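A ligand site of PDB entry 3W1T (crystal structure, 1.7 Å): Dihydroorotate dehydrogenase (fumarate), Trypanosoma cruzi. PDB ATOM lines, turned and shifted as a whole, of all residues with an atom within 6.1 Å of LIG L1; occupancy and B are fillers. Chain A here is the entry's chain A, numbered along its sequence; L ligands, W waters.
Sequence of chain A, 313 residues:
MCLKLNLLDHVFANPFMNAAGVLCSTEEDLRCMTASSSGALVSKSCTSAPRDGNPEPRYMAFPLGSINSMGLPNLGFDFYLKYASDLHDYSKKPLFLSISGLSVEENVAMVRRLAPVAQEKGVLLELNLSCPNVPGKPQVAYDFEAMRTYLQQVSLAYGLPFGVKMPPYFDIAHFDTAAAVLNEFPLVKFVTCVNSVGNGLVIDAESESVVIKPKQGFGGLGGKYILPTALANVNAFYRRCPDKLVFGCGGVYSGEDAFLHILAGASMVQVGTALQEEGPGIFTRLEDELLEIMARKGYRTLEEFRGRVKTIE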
ATOM      1  N   ALA A  20     -10.747   5.574   3.301  1.00  0.00           N
ATOM      2  CA  ALA A  20      -9.312   5.713   3.110  1.00  0.00           C
ATOM      3  C   ALA A  20      -8.653   5.923   4.484  1.00  0.00           C
ATOM      4  O   ALA A  20      -9.201   6.613   5.356  1.00  0.00           O
ATOM      5  CB  ALA A  20      -8.954   6.853   2.173  1.00  0.00           C
ATOM      6  N   LYS A  44      -4.688   3.633   1.158  1.00  0.00           N
ATOM      7  CA  LYS A  44      -4.287   4.750   1.972  1.00  0.00           C
ATOM      8  C   LYS A  44      -3.861   5.941   1.110  1.00  0.00           C
ATOM      9  O   LYS A  44      -3.034   5.779   0.215  1.00  0.00           O
ATOM     10  CB  LYS A  44      -3.114   4.346   2.838  1.00  0.00           C
ATOM     11  CG  LYS A  44      -2.513   5.434   3.707  1.00  0.00           C
ATOM     12  CD  LYS A  44      -3.397   5.991   4.783  1.00  0.00           C
ATOM     13  CE  LYS A  44      -2.880   7.318   5.433  1.00  0.00           C
ATOM     14  NZ  LYS A  44      -3.661   8.103   6.562  1.00  0.00           N
ATOM     15  N   SER A  45      -4.357   7.141   1.473  1.00  0.00           N
ATOM     16  CA  SER A  45      -3.960   8.397   0.815  1.00  0.00           C
ATOM     17  C   SER A  45      -2.470   8.419   0.819  1.00  0.00           C
ATOM     18  O   SER A  45      -1.841   8.210   1.853  1.00  0.00           O
ATOM     19  CB  SER A  45      -4.479   9.639   1.538  1.00  0.00           C
ATOM     20  OG  SER A  45      -5.890   9.661   1.348  1.00  0.00           O
ATOM     21  N   THR A  47       1.441  10.141  -0.610  1.00  0.00           N
ATOM     22  CA  THR A  47       2.348  11.219  -1.046  1.00  0.00           C
ATOM     23  C   THR A  47       3.391  10.621  -1.981  1.00  0.00           C
ATOM     24  O   THR A  47       3.535   9.397  -2.086  1.00  0.00           O
ATOM     25  CB  THR A  47       3.003  11.896   0.202  1.00  0.00           C
ATOM     26  OG1 THR A  47       3.516  10.916   1.097  1.00  0.00           O
ATOM     27  CG2 THR A  47       1.942  12.708   0.935  1.00  0.00           C
ATOM     28  N   ARG A  51       6.083   8.344   4.067  1.00  0.00           N
ATOM     29  CA  ARG A  51       6.050   9.063   5.294  1.00  0.00           C
ATOM     30  C   ARG A  51       5.826   8.151   6.505  1.00  0.00           C
ATOM     31  O   ARG A  51       5.042   7.256   6.468  1.00  0.00           O
ATOM     32  CB  ARG A  51       4.887  10.052   5.324  1.00  0.00           C
ATOM     33  CG  ARG A  51       4.975  11.177   4.338  1.00  0.00           C
ATOM     34  CD  ARG A  51       3.701  11.979   4.350  1.00  0.00           C
ATOM     35  NE  ARG A  51       3.378  12.553   5.625  1.00  0.00           N
ATOM     36  CZ  ARG A  51       3.782  13.738   6.026  1.00  0.00           C
ATOM     37  NH1 ARG A  51       4.556  14.433   5.222  1.00  0.00           N
ATOM     38  NH2 ARG A  51       3.451  14.189   7.212  1.00  0.00           N
ATOM     39  N   ASN A  54       3.060  10.924  12.215  1.00  0.00           N
ATOM     40  CA  ASN A  54       3.233  11.567  13.488  1.00  0.00           C
ATOM     41  C   ASN A  54       3.615  10.614  14.640  1.00  0.00           C
ATOM     42  O   ASN A  54       3.454   9.461  14.534  1.00  0.00           O
ATOM     43  CB  ASN A  54       1.973  12.346  13.895  1.00  0.00           C
ATOM     44  CG  ASN A  54       1.764  13.618  13.097  1.00  0.00           C
ATOM     45  OD1 ASN A  54       2.666  14.145  12.567  1.00  0.00           O
ATOM     46  ND2 ASN A  54       0.559  14.074  13.040  1.00  0.00           N
ATOM     47  N   ASN A  68      -8.044  11.183  15.525  1.00  0.00           N
ATOM     48  CA  ASN A  68      -6.728  10.891  14.982  1.00  0.00           C
ATOM     49  C   ASN A  68      -6.001  12.099  14.425  1.00  0.00           C
ATOM     50  O   ASN A  68      -6.603  13.002  13.883  1.00  0.00           O
ATOM     51  CB  ASN A  68      -6.840   9.822  13.869  1.00  0.00           C
ATOM     52  CG  ASN A  68      -7.114  10.431  12.509  1.00  0.00           C
ATOM     53  OD1 ASN A  68      -6.211  10.876  11.791  1.00  0.00           O
ATOM     54  ND2 ASN A  68      -8.338  10.381  12.104  1.00  0.00           N
ATOM     55  N   SER A  69      -4.690  12.088  14.554  1.00  0.00           N
ATOM     56  CA  SER A  69      -3.817  12.986  13.916  1.00  0.00           C
ATOM     57  C   SER A  69      -2.638  12.150  13.416  1.00  0.00           C
ATOM     58  O   SER A  69      -1.524  12.231  13.893  1.00  0.00           O
ATOM     59  CB  SER A  69      -3.412  14.152  14.783  1.00  0.00           C
ATOM     60  OG  SER A  69      -2.501  14.876  14.008  1.00  0.00           O
ATOM     61  N   MET A  70      -2.923  11.323  12.422  1.00  0.00           N
ATOM     62  CA  MET A  70      -1.925  10.352  11.992  1.00  0.00           C
ATOM     63  C   MET A  70      -0.718  10.958  11.274  1.00  0.00           C
ATOM     64  O   MET A  70       0.378  10.409  11.338  1.00  0.00           O
ATOM     65  CB  MET A  70      -2.544   9.405  11.039  1.00  0.00           C
ATOM     66  CG  MET A  70      -3.766   8.625  11.427  1.00  0.00           C
ATOM     67  SD  MET A  70      -3.558   7.547  12.796  1.00  0.00           S
ATOM     68  CE  MET A  70      -2.609   6.232  12.125  1.00  0.00           C
ATOM     69  N   GLY A  71      -0.897  12.097  10.614  1.00  0.00           N
ATOM     70  CA  GLY A  71       0.203  12.760   9.879  1.00  0.00           C
ATOM     71  C   GLY A  71       0.509  12.102   8.529  1.00  0.00           C
ATOM     72  O   GLY A  71       1.678  12.090   8.099  1.00  0.00           O
ATOM     73  N   LEU A  72      -0.467  11.426   7.959  1.00  0.00           N
ATOM     74  CA  LEU A  72      -0.367  10.819   6.638  1.00  0.00           C
ATOM     75  C   LEU A  72       0.787   9.822   6.519  1.00  0.00           C
ATOM     76  O   LEU A  72       1.524   9.833   5.507  1.00  0.00           O
ATOM     77  CB  LEU A  72      -0.358  11.888   5.546  1.00  0.00           C
ATOM     78  CG  LEU A  72      -0.664  11.582   4.073  1.00  0.00           C
ATOM     79  CD1 LEU A  72      -1.947  10.795   3.939  1.00  0.00           C
ATOM     80  CD2 LEU A  72      -0.784  13.000   3.442  1.00  0.00           C
ATOM     81  N   PRO A  73       0.938   8.874   7.434  1.00  0.00           N
ATOM     82  CA  PRO A  73       1.898   7.772   7.237  1.00  0.00           C
ATOM     83  C   PRO A  73       1.492   6.959   5.993  1.00  0.00           C
ATOM     84  O   PRO A  73       0.305   6.666   5.830  1.00  0.00           O
ATOM     85  CB  PRO A  73       1.749   6.926   8.513  1.00  0.00           C
ATOM     86  CG  PRO A  73       0.400   7.184   9.024  1.00  0.00           C
ATOM     87  CD  PRO A  73      -0.012   8.556   8.546  1.00  0.00           C
ATOM     88  N   SER A 100      -3.066  12.142  -1.784  1.00  0.00           N
ATOM     89  CA  SER A 100      -3.183  13.357  -0.998  1.00  0.00           C
ATOM     90  C   SER A 100      -1.866  14.112  -0.909  1.00  0.00           C
ATOM     91  O   SER A 100      -1.214  14.199   0.137  1.00  0.00           O
ATOM     92  CB  SER A 100      -3.687  12.959   0.419  1.00  0.00           C
ATOM     93  OG  SER A 100      -4.135  14.144   1.009  1.00  0.00           O
ATOM     94  N   LEU A 102       0.911  17.178  -0.924  1.00  0.00           N
ATOM     95  CA  LEU A 102       1.119  18.306  -0.022  1.00  0.00           C
ATOM     96  C   LEU A 102       1.119  19.628  -0.794  1.00  0.00           C
ATOM     97  O   LEU A 102       1.193  20.729  -0.173  1.00  0.00           O
ATOM     98  CB  LEU A 102       2.434  18.159   0.741  1.00  0.00           C
ATOM     99  CG  LEU A 102       2.582  16.840   1.567  1.00  0.00           C
ATOM    100  CD1 LEU A 102       3.826  16.839   2.479  1.00  0.00           C
ATOM    101  CD2 LEU A 102       1.386  16.536   2.357  1.00  0.00           C
ATOM    102  N   ASN A 128      -7.936  13.332  -2.287  1.00  0.00           N
ATOM    103  CA  ASN A 128      -8.263  13.809  -0.987  1.00  0.00           C
ATOM    104  C   ASN A 128      -7.951  15.315  -0.879  1.00  0.00           C
ATOM    105  O   ASN A 128      -6.828  15.710  -0.828  1.00  0.00           O
ATOM    106  CB  ASN A 128      -7.443  13.073   0.045  1.00  0.00           C
ATOM    107  CG  ASN A 128      -7.710  13.527   1.457  1.00  0.00           C
ATOM    108  OD1 ASN A 128      -8.546  14.249   1.715  1.00  0.00           O
ATOM    109  ND2 ASN A 128      -6.955  13.031   2.337  1.00  0.00           N
ATOM    110  N   SER A 130      -8.680  17.198   1.701  1.00  0.00           N
ATOM    111  CA  SER A 130      -8.234  17.638   3.041  1.00  0.00           C
ATOM    112  C   SER A 130      -6.721  17.833   3.195  1.00  0.00           C
ATOM    113  O   SER A 130      -6.234  18.048   4.203  1.00  0.00           O
ATOM    114  CB  SER A 130      -8.711  16.748   4.141  1.00  0.00           C
ATOM    115  OG  SER A 130     -10.118  16.889   4.306  1.00  0.00           O
ATOM    116  N   CYS A 131      -5.968  17.625   2.175  1.00  0.00           N
ATOM    117  CA  CYS A 131      -4.582  17.894   2.233  1.00  0.00           C
ATOM    118  C   CYS A 131      -4.449  19.383   2.802  1.00  0.00           C
ATOM    119  O   CYS A 131      -5.139  20.277   2.472  1.00  0.00           O
ATOM    120  CB  CYS A 131      -3.916  17.609   0.906  1.00  0.00           C
ATOM    121  SG  CYS A 131      -4.713  18.415  -0.508  1.00  0.00           S
ATOM    122  N   PRO A 132      -3.530  19.518   3.759  1.00  0.00           N
ATOM    123  CA  PRO A 132      -3.011  20.831   4.058  1.00  0.00           C
ATOM    124  C   PRO A 132      -2.346  21.340   2.818  1.00  0.00           C
ATOM    125  O   PRO A 132      -1.904  20.608   2.027  1.00  0.00           O
ATOM    126  CB  PRO A 132      -1.929  20.551   5.103  1.00  0.00           C
ATOM    127  CG  PRO A 132      -2.363  19.282   5.776  1.00  0.00           C
ATOM    128  CD  PRO A 132      -3.515  18.708   4.995  1.00  0.00           C
ATOM    129  N   LYS A 165     -12.565  13.367  -2.191  1.00  0.00           N
ATOM    130  CA  LYS A 165     -12.896  13.183  -0.773  1.00  0.00           C
ATOM    131  C   LYS A 165     -12.983  14.554  -0.078  1.00  0.00           C
ATOM    132  O   LYS A 165     -12.038  15.343  -0.171  1.00  0.00           O
ATOM    133  CB  LYS A 165     -11.865  12.302  -0.119  1.00  0.00           C
ATOM    134  CG  LYS A 165     -12.112  12.061   1.357  1.00  0.00           C
ATOM    135  CD  LYS A 165     -13.202  11.077   1.658  1.00  0.00           C
ATOM    136  CE  LYS A 165     -13.154  10.620   3.107  1.00  0.00           C
ATOM    137  NZ  LYS A 165     -12.045   9.701   3.402  1.00  0.00           N
ATOM    138  N   ASN A 195     -14.828  13.334   5.084  1.00  0.00           N
ATOM    139  CA  ASN A 195     -13.631  13.103   5.898  1.00  0.00           C
ATOM    140  C   ASN A 195     -13.952  13.446   7.377  1.00  0.00           C
ATOM    141  O   ASN A 195     -15.012  13.798   7.694  1.00  0.00           O
ATOM    142  CB  ASN A 195     -12.455  13.970   5.368  1.00  0.00           C
ATOM    143  CG  ASN A 195     -11.106  13.309   5.528  1.00  0.00           C
ATOM    144  OD1 ASN A 195     -10.829  12.863   6.535  1.00  0.00           O
ATOM    145  ND2 ASN A 195     -10.310  13.304   4.492  1.00  0.00           N
ATOM    146  N   SER A 196     -12.959  13.307   8.242  1.00  0.00           N
ATOM    147  CA  SER A 196     -13.226  13.439   9.653  1.00  0.00           C
ATOM    148  C   SER A 196     -13.627  14.864   9.988  1.00  0.00           C
ATOM    149  O   SER A 196     -13.338  15.758   9.266  1.00  0.00           O
ATOM    150  CB  SER A 196     -11.996  13.007  10.455  1.00  0.00           C
ATOM    151  OG  SER A 196     -10.887  13.589  10.032  1.00  0.00           O
ATOM    152  N   LYS A 215      -0.273  17.676  17.903  1.00  0.00           N
ATOM    153  CA  LYS A 215      -1.204  18.856  17.879  1.00  0.00           C
ATOM    154  C   LYS A 215      -1.876  19.128  19.239  1.00  0.00           C
ATOM    155  O   LYS A 215      -3.022  19.529  19.302  1.00  0.00           O
ATOM    156  CB  LYS A 215      -2.259  18.619  16.773  1.00  0.00           C
ATOM    157  CG  LYS A 215      -1.714  18.636  15.385  1.00  0.00           C
ATOM    158  CD  LYS A 215      -2.768  18.434  14.292  1.00  0.00           C
ATOM    159  CE  LYS A 215      -3.955  19.396  14.380  1.00  0.00           C
ATOM    160  NZ  LYS A 215      -4.808  19.146  13.185  1.00  0.00           N
ATOM    161  N   GLY A 220      -8.788  14.715  14.049  1.00  0.00           N
ATOM    162  CA  GLY A 220     -10.079  14.559  13.363  1.00  0.00           C
ATOM    163  C   GLY A 220     -10.956  13.476  14.012  1.00  0.00           C
ATOM    164  O   GLY A 220     -10.494  12.408  14.421  1.00  0.00           O
HETATM  165  O1  LIG L   1      -3.327  10.983   7.965  1.00  0.00           O
HETATM  166  C1  LIG L   1      -4.130  11.722   8.541  1.00  0.00           C
HETATM  167  O2  LIG L   1      -3.949  12.305   9.624  1.00  0.00           O
HETATM  168  C2  LIG L   1      -5.505  11.909   8.003  1.00  0.00           C
HETATM  169  N1  LIG L   1      -6.485  11.637   8.960  1.00  0.00           N
HETATM  170  C3  LIG L   1      -7.864  11.755   8.633  1.00  0.00           C
HETATM  171  O3  LIG L   1      -8.757  11.612   9.458  1.00  0.00           O
HETATM  172  N2  LIG L   1      -8.176  12.155   7.338  1.00  0.00           N
HETATM  173  C4  LIG L   1      -7.193  12.492   6.364  1.00  0.00           C
HETATM  174  O4  LIG L   1      -7.537  12.887   5.245  1.00  0.00           O
HETATM  175  C5  LIG L   1      -5.818  12.336   6.727  1.00  0.00           C
HETATM  176  C6  LIG L   1      -4.824  12.627   5.804  1.00  0.00           C
HETATM  177  C7  LIG L   1      -4.779  14.132   5.483  1.00  0.00           C
HETATM  178  C8  LIG L   1      -3.988  14.832   6.310  1.00  0.00           C
HETATM  179  C9  LIG L   1      -2.571  14.969   6.052  1.00  0.00           C
HETATM  180  C10 LIG L   1      -1.782  15.677   6.982  1.00  0.00           C
HETATM  181  C11 LIG L   1      -0.320  15.856   6.772  1.00  0.00           C
HETATM  182  F1  LIG L   1       0.180  15.647   5.678  1.00  0.00           F
HETATM  183  F2  LIG L   1      -0.045  17.014   6.986  1.00  0.00           F
HETATM  184  F3  LIG L   1       0.273  15.044   7.511  1.00  0.00           F
HETATM  185  C12 LIG L   1      -2.374  16.229   8.163  1.00  0.00           C
HETATM  186  C13 LIG L   1      -3.762  16.114   8.415  1.00  0.00           C
HETATM  187  C14 LIG L   1      -4.555  15.419   7.465  1.00  0.00           C
HETATM  188  N1  LG2 L   2      -9.310   9.985   4.952  1.00  0.00           N
HETATM  189  C1  LG2 L   2      -8.629  10.086   3.798  1.00  0.00           C
HETATM  190  O1  LG2 L   2      -9.257  10.536   2.815  1.00  0.00           O
HETATM  191  N2  LG2 L   2      -7.314   9.701   3.671  1.00  0.00           N
HETATM  192  C2  LG2 L   2      -6.638   9.150   4.684  1.00  0.00           C
HETATM  193  O2  LG2 L   2      -5.442   8.740   4.619  1.00  0.00           O
HETATM  194  C3  LG2 L   2      -7.328   8.922   5.944  1.00  0.00           C
HETATM  195  N3  LG2 L   2      -6.667   8.397   7.003  1.00  0.00           N
HETATM  196  C4  LG2 L   2      -7.382   8.111   8.112  1.00  0.00           C
HETATM  197  C5  LG2 L   2      -6.769   7.367   9.162  1.00  0.00           C
HETATM  198  C6  LG2 L   2      -7.442   7.022  10.302  1.00  0.00           C
HETATM  199  C7  LG2 L   2      -6.779   6.248  11.410  1.00  0.00           C
HETATM  200  C8  LG2 L   2      -8.848   7.361  10.402  1.00  0.00           C
HETATM  201  C9  LG2 L   2      -9.597   7.028  11.643  1.00  0.00           C
HETATM  202  C10 LG2 L   2      -9.467   8.092   9.385  1.00  0.00           C
HETATM  203  C11 LG2 L   2      -8.804   8.400   8.187  1.00  0.00           C
HETATM  204  N4  LG2 L   2      -9.393   9.158   7.171  1.00  0.00           N
HETATM  205  C12 LG2 L   2      -8.706   9.390   6.006  1.00  0.00           C
HETATM  206  C13 LG2 L   2     -10.806   9.559   7.246  1.00  0.00           C
HETATM  207  C14 LG2 L   2     -11.706   8.382   7.014  1.00  0.00           C
HETATM  208  O3  LG2 L   2     -11.562   8.013   5.690  1.00  0.00           O
HETATM  209  C15 LG2 L   2     -13.109   8.828   7.213  1.00  0.00           C
HETATM  210  O4  LG2 L   2     -13.446   9.877   6.280  1.00  0.00           O
HETATM  211  C16 LG2 L   2     -13.457   9.296   8.654  1.00  0.00           C
HETATM  212  O5  LG2 L   2     -12.801   8.450   9.582  1.00  0.00           O
HETATM  213  C17 LG2 L   2     -14.969   9.191   8.922  1.00  0.00           C
HETATM  214  O6  LG2 L   2     -15.602   7.904   8.722  1.00  0.00           O
HETATM  215  P1  LG2 L   2     -15.922   7.067  10.059  1.00  0.00           P
HETATM  216  O7  LG2 L   2     -16.429   5.755   9.529  1.00  0.00           O
HETATM  217  O8  LG2 L   2     -16.927   7.836  10.856  1.00  0.00           O
HETATM  218  O9  LG2 L   2     -14.606   6.890  10.817  1.00  0.00           O
HETATM  219  O   HOH W   1      -2.557  14.584  11.286  1.00  0.00           O
HETATM  220  O   HOH W   2      -6.183  14.090  11.092  1.00  0.00           O
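The backbone NH of Gly 71 lies within hydrogen-bond range of an oxygen (O2) of LIG L1.
The side-chain hydroxyl of Ser 196 is in hydrogen-bond range of an oxygen (O3) of LIG L1.
An oxygen (O4) of LIG L1 is in hydrogen-bond range of the side-chain amide nitrogen (ND2) of Asn 128, 3.0 Å away.
O of Ala 20 sits at hydrogen-bond distance from O3 of LG2 L2.
The side-chain amide nitrogen of Asn 128 lies within hydrogen-bond range of an oxygen (O1) of LG2 L2.
A nitrogen (N2) of LIG L1 lies within hydrogen-bond range of the side-chain amide oxygen (OD1) of Asn 195 (2.9 Å).
NZ of Lys 44 lies within salt-bridge range of O1 of LIG L1, at 3.2 Å.
An oxygen (O3) of LG2 L2 is in hydrogen-bond range of the side-chain amino group of Lys 165 (2.9 Å).
A nitrogen (N1) of LIG L1 is in hydrogen-bond range of the side-chain amide oxygen (OD1) of Asn 68, at 2.9 Å.
O2 of LIG L1 lies within hydrogen-bond range of N of Met 70 (3.1 Å).
The side-chain amide nitrogen of Asn 195 lies within hydrogen-bond range of an oxygen (O1) of LG2 L2, 3.4 Å away.
An oxygen (O1) of LIG L1 sits at hydrogen-bond distance from the backbone NH (N) of Leu 72 (2.9 Å).
The side-chain hydroxyl (OG) of Ser 45 sits at hydrogen-bond distance from a nitrogen (N2) of LG2 L2, at 2.7 Å.
The side-chain amino group of Lys 44 is in hydrogen-bond range of an oxygen (O2) of LG2 L2.
A nitrogen (N2) of LIG L1 lies close to a nitrogen (N1) of LG2 L2 (3.4 Å).
OD1 of Asn 68 sits close to N of Met 70 (3.4 Å).
The backbone carbonyl oxygen (O) of Leu 72 sits close to the guanidinium group (NE) of Arg 51.
The backbone NH of Gly 71 sits close to the side-chain amide nitrogen of Asn 54, 3.5 Å away.
NH2 of Arg 51 lies within hydrogen-bond range of O of Gly 71 (2.9 Å).
ND2 of Asn 128 lies within hydrogen-bond range of OG of Ser 100.
O of Asn 68 is in hydrogen-bond range of N of Gly 220.
The backbone carbonyl oxygen of Asn 128 sits at hydrogen-bond distance from the side-chain sulfur of Cys 131 (3.4 Å).
O of Met 70 sits at hydrogen-bond distance from N of Asn 54, 2.9 Å away.
A fluorine (F3) of LIG L1 lies close to the guanidinium group of Arg 51 (3.3 Å).
Leu 102 touches LIG L1 (CD2 to F1, 3.6 Å).
CG of Pro 132 touches F2 of LIG L1 (3.5 Å).
Hydrophobic or aromatic side chains that line LIG L1: Met 70, Leu 72, Leu 102 and Pro 132.
11 residues have an atom within 4 Å of LIG L1: Lys 44, Arg 51, Asn 68, Met 70, Gly 71, Leu 72, Leu 102, Asn 128, Pro 132, Asn 195 and Ser 196.
Water W1 lies within hydrogen-bond range of the side-chain hydroxyl (OG) of Ser 69 (2.7 Å), the backbone NH (N) of Gly 71 (3.1 Å), an oxygen (O2) of LIG L1 (3.1 Å) and the backbone NH (N) of Met 70 (3.5 Å).
Water W2 bridges O of Asn 68 (3.0 Å) and O2 of LIG L1 (3.2 Å).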
